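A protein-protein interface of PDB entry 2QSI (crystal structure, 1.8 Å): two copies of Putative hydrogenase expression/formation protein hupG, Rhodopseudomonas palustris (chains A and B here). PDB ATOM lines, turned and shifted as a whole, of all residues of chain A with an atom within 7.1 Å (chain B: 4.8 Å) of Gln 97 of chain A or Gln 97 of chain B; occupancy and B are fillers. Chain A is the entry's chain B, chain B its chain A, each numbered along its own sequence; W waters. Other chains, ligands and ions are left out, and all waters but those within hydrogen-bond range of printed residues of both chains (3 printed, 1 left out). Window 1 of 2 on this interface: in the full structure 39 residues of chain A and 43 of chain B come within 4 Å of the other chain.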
ATOM      1  N   ILE A  29       5.108   7.067  23.047  1.00  0.00           N
ATOM      2  CA  ILE A  29       5.722   5.787  22.695  1.00  0.00           C
ATOM      3  C   ILE A  29       5.108   4.541  23.359  1.00  0.00           C
ATOM      4  O   ILE A  29       5.505   3.436  23.026  1.00  0.00           O
ATOM      5  CB  ILE A  29       7.195   5.793  22.993  1.00  0.00           C
ATOM      6  CG1 ILE A  29       7.439   5.916  24.516  1.00  0.00           C
ATOM      7  CG2 ILE A  29       7.859   6.938  22.261  1.00  0.00           C
ATOM      8  CD1 ILE A  29       8.944   5.933  24.910  1.00  0.00           C
ATOM      9  N   LYS A  34       7.914  -1.119  19.587  1.00  0.00           N
ATOM     10  CA  LYS A  34       8.935  -0.683  18.636  1.00  0.00           C
ATOM     11  C   LYS A  34      10.100  -0.007  19.368  1.00  0.00           C
ATOM     12  O   LYS A  34      10.039   0.259  20.573  1.00  0.00           O
ATOM     13  CB  LYS A  34       8.326   0.267  17.616  1.00  0.00           C
ATOM     14  CG  LYS A  34       7.338  -0.451  16.689  1.00  0.00           C
ATOM     15  CD  LYS A  34       6.672   0.471  15.744  1.00  0.00           C
ATOM     16  CE  LYS A  34       5.546  -0.258  14.996  1.00  0.00           C
ATOM     17  NZ  LYS A  34       5.077   0.519  13.822  1.00  0.00           N
ATOM     18  N   ILE A  35      11.166   0.220  18.607  1.00  0.00           N
ATOM     19  CA  ILE A  35      12.342   0.938  19.058  1.00  0.00           C
ATOM     20  C   ILE A  35      12.085   2.379  18.655  1.00  0.00           C
ATOM     21  O   ILE A  35      11.621   2.645  17.545  1.00  0.00           O
ATOM     22  CB  ILE A  35      13.629   0.356  18.440  1.00  0.00           C
ATOM     23  CG1 ILE A  35      13.856  -1.113  18.906  1.00  0.00           C
ATOM     24  CG2 ILE A  35      14.883   1.233  18.753  1.00  0.00           C
ATOM     25  CD1 ILE A  35      14.005  -1.252  20.393  1.00  0.00           C
ATOM     26  N   VAL A  36      12.403   3.305  19.564  1.00  0.00           N
ATOM     27  CA  VAL A  36      12.093   4.695  19.397  1.00  0.00           C
ATOM     28  C   VAL A  36      13.328   5.429  18.881  1.00  0.00           C
ATOM     29  O   VAL A  36      14.402   5.148  19.355  1.00  0.00           O
ATOM     30  CB  VAL A  36      11.708   5.357  20.764  1.00  0.00           C
ATOM     31  CG1 VAL A  36      11.346   6.859  20.519  1.00  0.00           C
ATOM     32  CG2 VAL A  36      10.542   4.612  21.437  1.00  0.00           C
ATOM     33  N   PHE A  85      18.301  10.495  28.181  1.00  0.00           N
ATOM     34  CA  PHE A  85      18.749   9.446  27.240  1.00  0.00           C
ATOM     35  C   PHE A  85      20.252   9.351  26.988  1.00  0.00           C
ATOM     36  O   PHE A  85      20.708   8.473  26.266  1.00  0.00           O
ATOM     37  CB  PHE A  85      17.922   9.585  25.950  1.00  0.00           C
ATOM     38  CG  PHE A  85      16.454   9.312  26.165  1.00  0.00           C
ATOM     39  CD1 PHE A  85      16.039   8.046  26.555  1.00  0.00           C
ATOM     40  CD2 PHE A  85      15.505  10.317  26.074  1.00  0.00           C
ATOM     41  CE1 PHE A  85      14.696   7.779  26.775  1.00  0.00           C
ATOM     42  CE2 PHE A  85      14.166  10.036  26.302  1.00  0.00           C
ATOM     43  CZ  PHE A  85      13.777   8.778  26.660  1.00  0.00           C
ATOM     44  N   VAL A  95      18.546   6.310  19.780  1.00  0.00           N
ATOM     45  CA  VAL A  95      17.845   5.074  19.453  1.00  0.00           C
ATOM     46  C   VAL A  95      17.671   4.336  20.779  1.00  0.00           C
ATOM     47  O   VAL A  95      18.674   3.992  21.443  1.00  0.00           O
ATOM     48  CB  VAL A  95      18.610   4.236  18.451  1.00  0.00           C
ATOM     49  CG1 VAL A  95      17.776   2.975  18.013  1.00  0.00           C
ATOM     50  CG2 VAL A  95      19.001   5.098  17.198  1.00  0.00           C
ATOM     51  N   VAL A  96      16.405   4.197  21.182  1.00  0.00           N
ATOM     52  CA  VAL A  96      16.013   3.867  22.558  1.00  0.00           C
ATOM     53  C   VAL A  96      15.071   2.648  22.590  1.00  0.00           C
ATOM     54  O   VAL A  96      14.073   2.615  21.854  1.00  0.00           O
ATOM     55  CB  VAL A  96      15.312   5.075  23.233  1.00  0.00           C
ATOM     56  CG1 VAL A  96      14.800   4.734  24.668  1.00  0.00           C
ATOM     57  CG2 VAL A  96      16.236   6.290  23.282  1.00  0.00           C
ATOM     58  N   GLN A  97      15.446   1.624  23.359  1.00  0.00           N
ATOM     59  CA  GLN A  97      14.523   0.514  23.703  1.00  0.00           C
ATOM     60  C   GLN A  97      13.653   1.033  24.844  1.00  0.00           C
ATOM     61  O   GLN A  97      14.150   1.259  25.946  1.00  0.00           O
ATOM     62  CB  GLN A  97      15.282  -0.725  24.181  1.00  0.00           C
ATOM     63  CG  GLN A  97      14.435  -2.013  24.262  1.00  0.00           C
ATOM     64  CD  GLN A  97      15.320  -3.259  24.294  1.00  0.00           C
ATOM     65  OE1 GLN A  97      16.398  -3.248  24.899  1.00  0.00           O
ATOM     66  NE2 GLN A  97      14.900  -4.315  23.598  1.00  0.00           N
ATOM     67  N   PRO A  98      12.367   1.291  24.577  1.00  0.00           N
ATOM     68  CA  PRO A  98      11.544   1.843  25.645  1.00  0.00           C
ATOM     69  C   PRO A  98      11.261   0.878  26.811  1.00  0.00           C
ATOM     70  O   PRO A  98      11.349  -0.360  26.680  1.00  0.00           O
ATOM     71  CB  PRO A  98      10.244   2.247  24.944  1.00  0.00           C
ATOM     72  CG  PRO A  98      10.262   1.603  23.613  1.00  0.00           C
ATOM     73  CD  PRO A  98      11.643   1.116  23.312  1.00  0.00           C
ATOM     74  N   GLU A  99      10.897   1.478  27.931  1.00  0.00           N
ATOM     75  CA  GLU A  99      10.498   0.724  29.107  1.00  0.00           C
ATOM     76  C   GLU A  99       9.309  -0.138  28.739  1.00  0.00           C
ATOM     77  O   GLU A  99       8.388   0.315  28.011  1.00  0.00           O
ATOM     78  CB  GLU A  99      10.090   1.698  30.196  1.00  0.00           C
ATOM     79  CG  GLU A  99       9.723   1.104  31.491  1.00  0.00           C
ATOM     80  CD  GLU A  99       9.418   2.160  32.525  1.00  0.00           C
ATOM     81  OE1 GLU A  99      10.379   2.660  33.150  1.00  0.00           O
ATOM     82  OE2 GLU A  99       8.223   2.487  32.710  1.00  0.00           O
ATOM     83  N   ARG A 100       9.327  -1.382  29.178  1.00  0.00           N
ATOM     84  CA  ARG A 100       8.177  -2.246  28.955  1.00  0.00           C
ATOM     85  C   ARG A 100       7.990  -3.317  29.990  1.00  0.00           C
ATOM     86  O   ARG A 100       8.951  -3.765  30.633  1.00  0.00           O
ATOM     87  CB  ARG A 100       8.320  -2.882  27.591  1.00  0.00           C
ATOM     88  CG  ARG A 100       9.472  -3.795  27.481  1.00  0.00           C
ATOM     89  CD  ARG A 100       9.481  -4.433  26.110  1.00  0.00           C
ATOM     90  NE  ARG A 100      10.804  -4.930  25.788  1.00  0.00           N
ATOM     91  CZ  ARG A 100      11.111  -6.167  25.456  1.00  0.00           C
ATOM     92  NH1 ARG A 100      10.189  -7.116  25.405  1.00  0.00           N
ATOM     93  NH2 ARG A 100      12.375  -6.457  25.192  1.00  0.00           N
ATOM     94  N   THR A 101       6.752  -3.763  30.126  1.00  0.00           N
ATOM     95  CA  THR A 101       6.444  -4.854  31.068  1.00  0.00           C
ATOM     96  C   THR A 101       6.694  -6.176  30.386  1.00  0.00           C
ATOM     97  O   THR A 101       6.140  -6.437  29.325  1.00  0.00           O
ATOM     98  CB  THR A 101       4.980  -4.780  31.579  1.00  0.00           C
ATOM     99  OG1 THR A 101       4.802  -3.504  32.230  1.00  0.00           O
ATOM    100  CG2 THR A 101       4.667  -5.915  32.577  1.00  0.00           C
ATOM    101  N   LEU A 102       7.579  -6.973  30.957  1.00  0.00           N
ATOM    102  CA  LEU A 102       7.896  -8.326  30.429  1.00  0.00           C
ATOM    103  C   LEU A 102       6.856  -9.361  30.792  1.00  0.00           C
ATOM    104  O   LEU A 102       6.685 -10.357  30.085  1.00  0.00           O
ATOM    105  CB  LEU A 102       9.257  -8.806  30.951  1.00  0.00           C
ATOM    106  CG  LEU A 102      10.459  -7.919  30.636  1.00  0.00           C
ATOM    107  CD1 LEU A 102      11.731  -8.575  31.175  1.00  0.00           C
ATOM    108  CD2 LEU A 102      10.580  -7.623  29.147  1.00  0.00           C
ATOM    109  N   MET A 121      10.985 -15.242  31.361  1.00  0.00           N
ATOM    110  CA  MET A 121      11.037 -13.869  30.894  1.00  0.00           C
ATOM    111  C   MET A 121      12.485 -13.476  30.637  1.00  0.00           C
ATOM    112  O   MET A 121      12.778 -12.785  29.629  1.00  0.00           O
ATOM    113  CB  MET A 121      10.410 -12.928  31.905  1.00  0.00           C
ATOM    114  CG  MET A 121       8.942 -13.181  32.118  1.00  0.00           C
ATOM    115  SD  MET A 121       8.285 -11.977  33.485  1.00  0.00           S
ATOM    116  CE  MET A 121       7.009 -13.218  34.236  1.00  0.00           C
ATOM    117  N   VAL A 125      14.387 -12.315  27.089  1.00  0.00           N
ATOM    118  CA  VAL A 125      15.294 -11.160  27.017  1.00  0.00           C
ATOM    119  C   VAL A 125      16.639 -11.511  26.418  1.00  0.00           C
ATOM    120  O   VAL A 125      17.137 -10.799  25.548  1.00  0.00           O
ATOM    121  CB  VAL A 125      15.528 -10.516  28.385  1.00  0.00           C
ATOM    122  CG1 VAL A 125      16.638  -9.460  28.307  1.00  0.00           C
ATOM    123  CG2 VAL A 125      14.233  -9.920  28.869  1.00  0.00           C
ATOM    124  N   ASP A 126      17.211 -12.625  26.857  1.00  0.00           N
ATOM    125  CA  ASP A 126      18.570 -12.992  26.444  1.00  0.00           C
ATOM    126  C   ASP A 126      18.641 -13.584  25.034  1.00  0.00           C
ATOM    127  O   ASP A 126      19.697 -13.537  24.402  1.00  0.00           O
ATOM    128  CB  ASP A 126      19.153 -13.982  27.440  1.00  0.00           C
ATOM    129  CG  ASP A 126      19.359 -13.382  28.806  1.00  0.00           C
ATOM    130  OD1 ASP A 126      19.407 -12.130  28.957  1.00  0.00           O
ATOM    131  OD2 ASP A 126      19.496 -14.182  29.745  1.00  0.00           O
ATOM    132  N   ILE B  35      16.610  -5.667  35.638  1.00  0.00           N
ATOM    133  CA  ILE B  35      15.160  -5.840  35.444  1.00  0.00           C
ATOM    134  C   ILE B  35      14.526  -5.634  36.824  1.00  0.00           C
ATOM    135  O   ILE B  35      15.027  -6.145  37.839  1.00  0.00           O
ATOM    136  CB  ILE B  35      14.833  -7.253  34.883  1.00  0.00           C
ATOM    137  CG1 ILE B  35      15.346  -7.457  33.426  1.00  0.00           C
ATOM    138  CG2 ILE B  35      13.351  -7.571  34.954  1.00  0.00           C
ATOM    139  CD1 ILE B  35      15.089  -6.324  32.549  1.00  0.00           C
ATOM    140  N   VAL B  95       7.039  -7.510  36.191  1.00  0.00           N
ATOM    141  CA  VAL B  95       8.450  -7.571  35.807  1.00  0.00           C
ATOM    142  C   VAL B  95       8.659  -6.571  34.669  1.00  0.00           C
ATOM    143  O   VAL B  95       8.051  -6.703  33.584  1.00  0.00           O
ATOM    144  CB  VAL B  95       8.858  -8.976  35.411  1.00  0.00           C
ATOM    145  CG1 VAL B  95      10.364  -9.036  35.127  1.00  0.00           C
ATOM    146  CG2 VAL B  95       8.462  -9.971  36.519  1.00  0.00           C
ATOM    147  N   VAL B  96       9.513  -5.586  34.909  1.00  0.00           N
ATOM    148  CA  VAL B  96       9.619  -4.418  34.025  1.00  0.00           C
ATOM    149  C   VAL B  96      11.064  -4.217  33.559  1.00  0.00           C
ATOM    150  O   VAL B  96      11.965  -4.124  34.389  1.00  0.00           O
ATOM    151  CB  VAL B  96       9.192  -3.138  34.748  1.00  0.00           C
ATOM    152  CG1 VAL B  96       9.372  -1.940  33.828  1.00  0.00           C
ATOM    153  CG2 VAL B  96       7.728  -3.205  35.244  1.00  0.00           C
ATOM    154  N   GLN B  97      11.269  -4.081  32.257  1.00  0.00           N
ATOM    155  CA  GLN B  97      12.573  -3.794  31.726  1.00  0.00           C
ATOM    156  C   GLN B  97      12.712  -2.276  31.565  1.00  0.00           C
ATOM    157  O   GLN B  97      11.898  -1.649  30.885  1.00  0.00           O
ATOM    158  CB  GLN B  97      12.715  -4.481  30.379  1.00  0.00           C
ATOM    159  CG  GLN B  97      14.047  -4.392  29.797  1.00  0.00           C
ATOM    160  CD  GLN B  97      14.133  -5.178  28.536  1.00  0.00           C
ATOM    161  OE1 GLN B  97      13.570  -4.795  27.527  1.00  0.00           O
ATOM    162  NE2 GLN B  97      14.864  -6.269  28.574  1.00  0.00           N
ATOM    163  N   PRO B  98      13.738  -1.684  32.216  1.00  0.00           N
ATOM    164  CA  PRO B  98      13.968  -0.262  32.067  1.00  0.00           C
ATOM    165  C   PRO B  98      14.265   0.137  30.635  1.00  0.00           C
ATOM    166  O   PRO B  98      14.840  -0.662  29.851  1.00  0.00           O
ATOM    167  CB  PRO B  98      15.179   0.001  32.932  1.00  0.00           C
ATOM    168  CG  PRO B  98      15.309  -1.119  33.849  1.00  0.00           C
ATOM    169  CD  PRO B  98      14.694  -2.301  33.155  1.00  0.00           C
ATOM    170  N   GLU B  99      14.043   1.406  30.347  1.00  0.00           N
ATOM    171  CA  GLU B  99      14.429   1.928  29.031  1.00  0.00           C
ATOM    172  C   GLU B  99      15.955   1.868  28.905  1.00  0.00           C
ATOM    173  O   GLU B  99      16.671   1.934  29.917  1.00  0.00           O
ATOM    174  CB  GLU B  99      13.897   3.326  28.815  1.00  0.00           C
ATOM    175  CG  GLU B  99      14.506   4.395  29.684  1.00  0.00           C
ATOM    176  CD  GLU B  99      13.829   5.744  29.501  1.00  0.00           C
ATOM    177  OE1 GLU B  99      12.769   5.822  28.785  1.00  0.00           O
ATOM    178  OE2 GLU B  99      14.381   6.725  30.045  1.00  0.00           O
ATOM    179  N   ARG B 100      16.446   1.761  27.662  1.00  0.00           N
ATOM    180  CA  ARG B 100      17.893   1.699  27.428  1.00  0.00           C
ATOM    181  C   ARG B 100      18.190   2.399  26.130  1.00  0.00           C
ATOM    182  O   ARG B 100      17.528   2.164  25.120  1.00  0.00           O
ATOM    183  CB  ARG B 100      18.393   0.245  27.396  1.00  0.00           C
ATOM    184  CG  ARG B 100      19.896   0.058  27.342  1.00  0.00           C
ATOM    185  CD  ARG B 100      20.234  -1.404  26.999  1.00  0.00           C
ATOM    186  NE  ARG B 100      21.278  -1.454  25.966  1.00  0.00           N
ATOM    187  CZ  ARG B 100      21.362  -2.384  25.011  1.00  0.00           C
ATOM    188  NH1 ARG B 100      20.463  -3.367  24.919  1.00  0.00           N
ATOM    189  NH2 ARG B 100      22.348  -2.329  24.131  1.00  0.00           N
ATOM    190  N   LEU B 102      20.168   2.438  23.070  1.00  0.00           N
ATOM    191  CA  LEU B 102      20.945   1.476  22.311  1.00  0.00           C
ATOM    192  C   LEU B 102      22.153   2.144  21.641  1.00  0.00           C
ATOM    193  O   LEU B 102      23.173   1.514  21.387  1.00  0.00           O
ATOM    194  CB  LEU B 102      20.071   0.806  21.250  1.00  0.00           C
ATOM    195  CG  LEU B 102      18.851   0.062  21.800  1.00  0.00           C
ATOM    196  CD1 LEU B 102      18.012  -0.412  20.605  1.00  0.00           C
ATOM    197  CD2 LEU B 102      19.210  -1.095  22.787  1.00  0.00           C
ATOM    198  N   VAL B 125      19.510  -6.110  19.570  1.00  0.00           N
ATOM    199  CA  VAL B 125      18.204  -6.378  20.184  1.00  0.00           C
ATOM    200  C   VAL B 125      17.764  -7.819  19.891  1.00  0.00           C
ATOM    201  O   VAL B 125      17.371  -8.543  20.804  1.00  0.00           O
ATOM    202  CB  VAL B 125      17.129  -5.342  19.733  1.00  0.00           C
ATOM    203  CG1 VAL B 125      15.726  -5.790  20.065  1.00  0.00           C
ATOM    204  CG2 VAL B 125      17.397  -4.007  20.395  1.00  0.00           C
HETATM  205  O   HOH W   1      12.872   3.130  32.305  1.00  0.00           O
HETATM  206  O   HOH W   2      16.660  -8.768  23.895  1.00  0.00           O
HETATM  207  O   HOH W   3      10.674   4.337  27.911  1.00  0.00           O
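The backbone carbonyl oxygen of Val 95 of chain A is in hydrogen-bond range of the backbone NH of Leu 102 of chain B (2.7 Å).
The backbone carbonyl oxygen (O) of Arg 100 of chain B sits at hydrogen-bond distance from the backbone NH (N) of Gln 97 of chain A (2.8 Å).
O of Arg 100 of chain A lies within hydrogen-bond range of N of Gln 97 of chain B (2.8 Å).
O of Val 95 of chain B lies within hydrogen-bond range of N of Leu 102 of chain A (2.7 Å).
The backbone carbonyl oxygen (O) of Val 36 of chain A lies within hydrogen-bond range of the backbone NH (N) of Val 96 of chain A (2.9 Å).
Ile 35 of chain A touches Leu 102 of chain B (CG2 to CD1, 3.99 Å).
Arg 100 of chain B touches Val 96 of chain A (O to CA, 3.4 Å).
Gln 97 of chain A touches Gln 97 of chain B (CD to OE1, 3.98 Å).
NE2 of Gln 97 of chain A touches CG1 of Val 125 of chain B, 3.9 Å away.
Val 96 of chain B touches Glu 99 of chain A.
Glu 99 of chain A touches Gln 97 of chain B (CA to O, 3.3 Å).
N of Glu 99 of chain A touches CB of Glu 99 of chain B, at 3.6 Å.
O of Arg 100 of chain A touches CA of Val 96 of chain B, 3.5 Å away.
CA of Thr 101 of chain A touches O of Val 95 of chain B, at 3.5 Å.
NE2 of Gln 97 of chain B touches CG1 of Val 125 of chain A, at 3.7 Å.
Of the printed residues of chain B, Ile 35 of chain A touches Leu 102.
Of the printed residues of chain B, Val 95 of chain A touches Leu 102.
Of the printed residues of chain B, Gln 97 of chain A touches Gln 97, Glu 99, Arg 100 and Val 125.
Of the printed residues of chain A, Val 95 of chain B touches Thr 101 (3.5 Å), Leu 102 (2.7 Å) and Met 121 (3.6 Å).
Printed residues of chain A within 4 Å of Gln 97 of chain B: Gln 97, Glu 99, Arg 100, Leu 102 and Val 125.
Of the printed residues of chain A, Glu 99 of chain B touches Phe 85 (3.4 Å), Gln 97 (3.2 Å) and Glu 99 (3.6 Å).
Printed residues of chain A within 4 Å of Val 125 of chain B: Gln 97.
The nearest printed residue of chain B that does not touch Gln 97 of chain A is Leu 102 of chain B (4.1 Å).
Of the 9 printed residues of chain B, 7 touch a printed residue of chain A.
Hydrophobic or aromatic side chains of chain A that line the printed part of chain B: Ile 35, Phe 85, Val 96, Leu 102, Met 121 and Val 125.
Among the printed residues, 18 pairs touch across the chains.
Among the printed residues, no Asp or Glu carboxylate lies within 4 Å of a Lys or Arg side-chain nitrogen of the other chain.
Val 95 of chain A touches Leu 102 of chain B, and with the chains exchanged Leu 102 of chain A touches Val 95 of chain B.
Val 96 of chain A touches Arg 100 of chain B, and with the chains exchanged Arg 100 of chain A touches Val 96 of chain B.
Gln 97 of chain B touches its own counterpart, Gln 97 of chain A.
Glu 99 of chain A touches Val 96 of chain B, but with the chains exchanged Val 96 of chain A does not touch Glu 99 of chain B (4.5 Å).
9 positions are printed for both chains.
Of the 18 pairs that touch across the chains among the printed residues, 12 have their exchanged pair printed and touching as well.
Water W2 lies within hydrogen-bond range of the backbone carbonyl oxygen of Val 125 of chain A (2.7 Å) and the backbone carbonyl oxygen of Val 125 of chain B (3.2 Å).
Water W1 lies within hydrogen-bond range of the side-chain carboxylate (OE1) of Glu 99 of chain A and the backbone NH (N) of Glu 99 of chain B.
Water W3 bridges the side-chain carboxylate of Glu 99 of chain B (2.7 Å) and the backbone NH of Glu 99 of chain A (2.9 Å).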
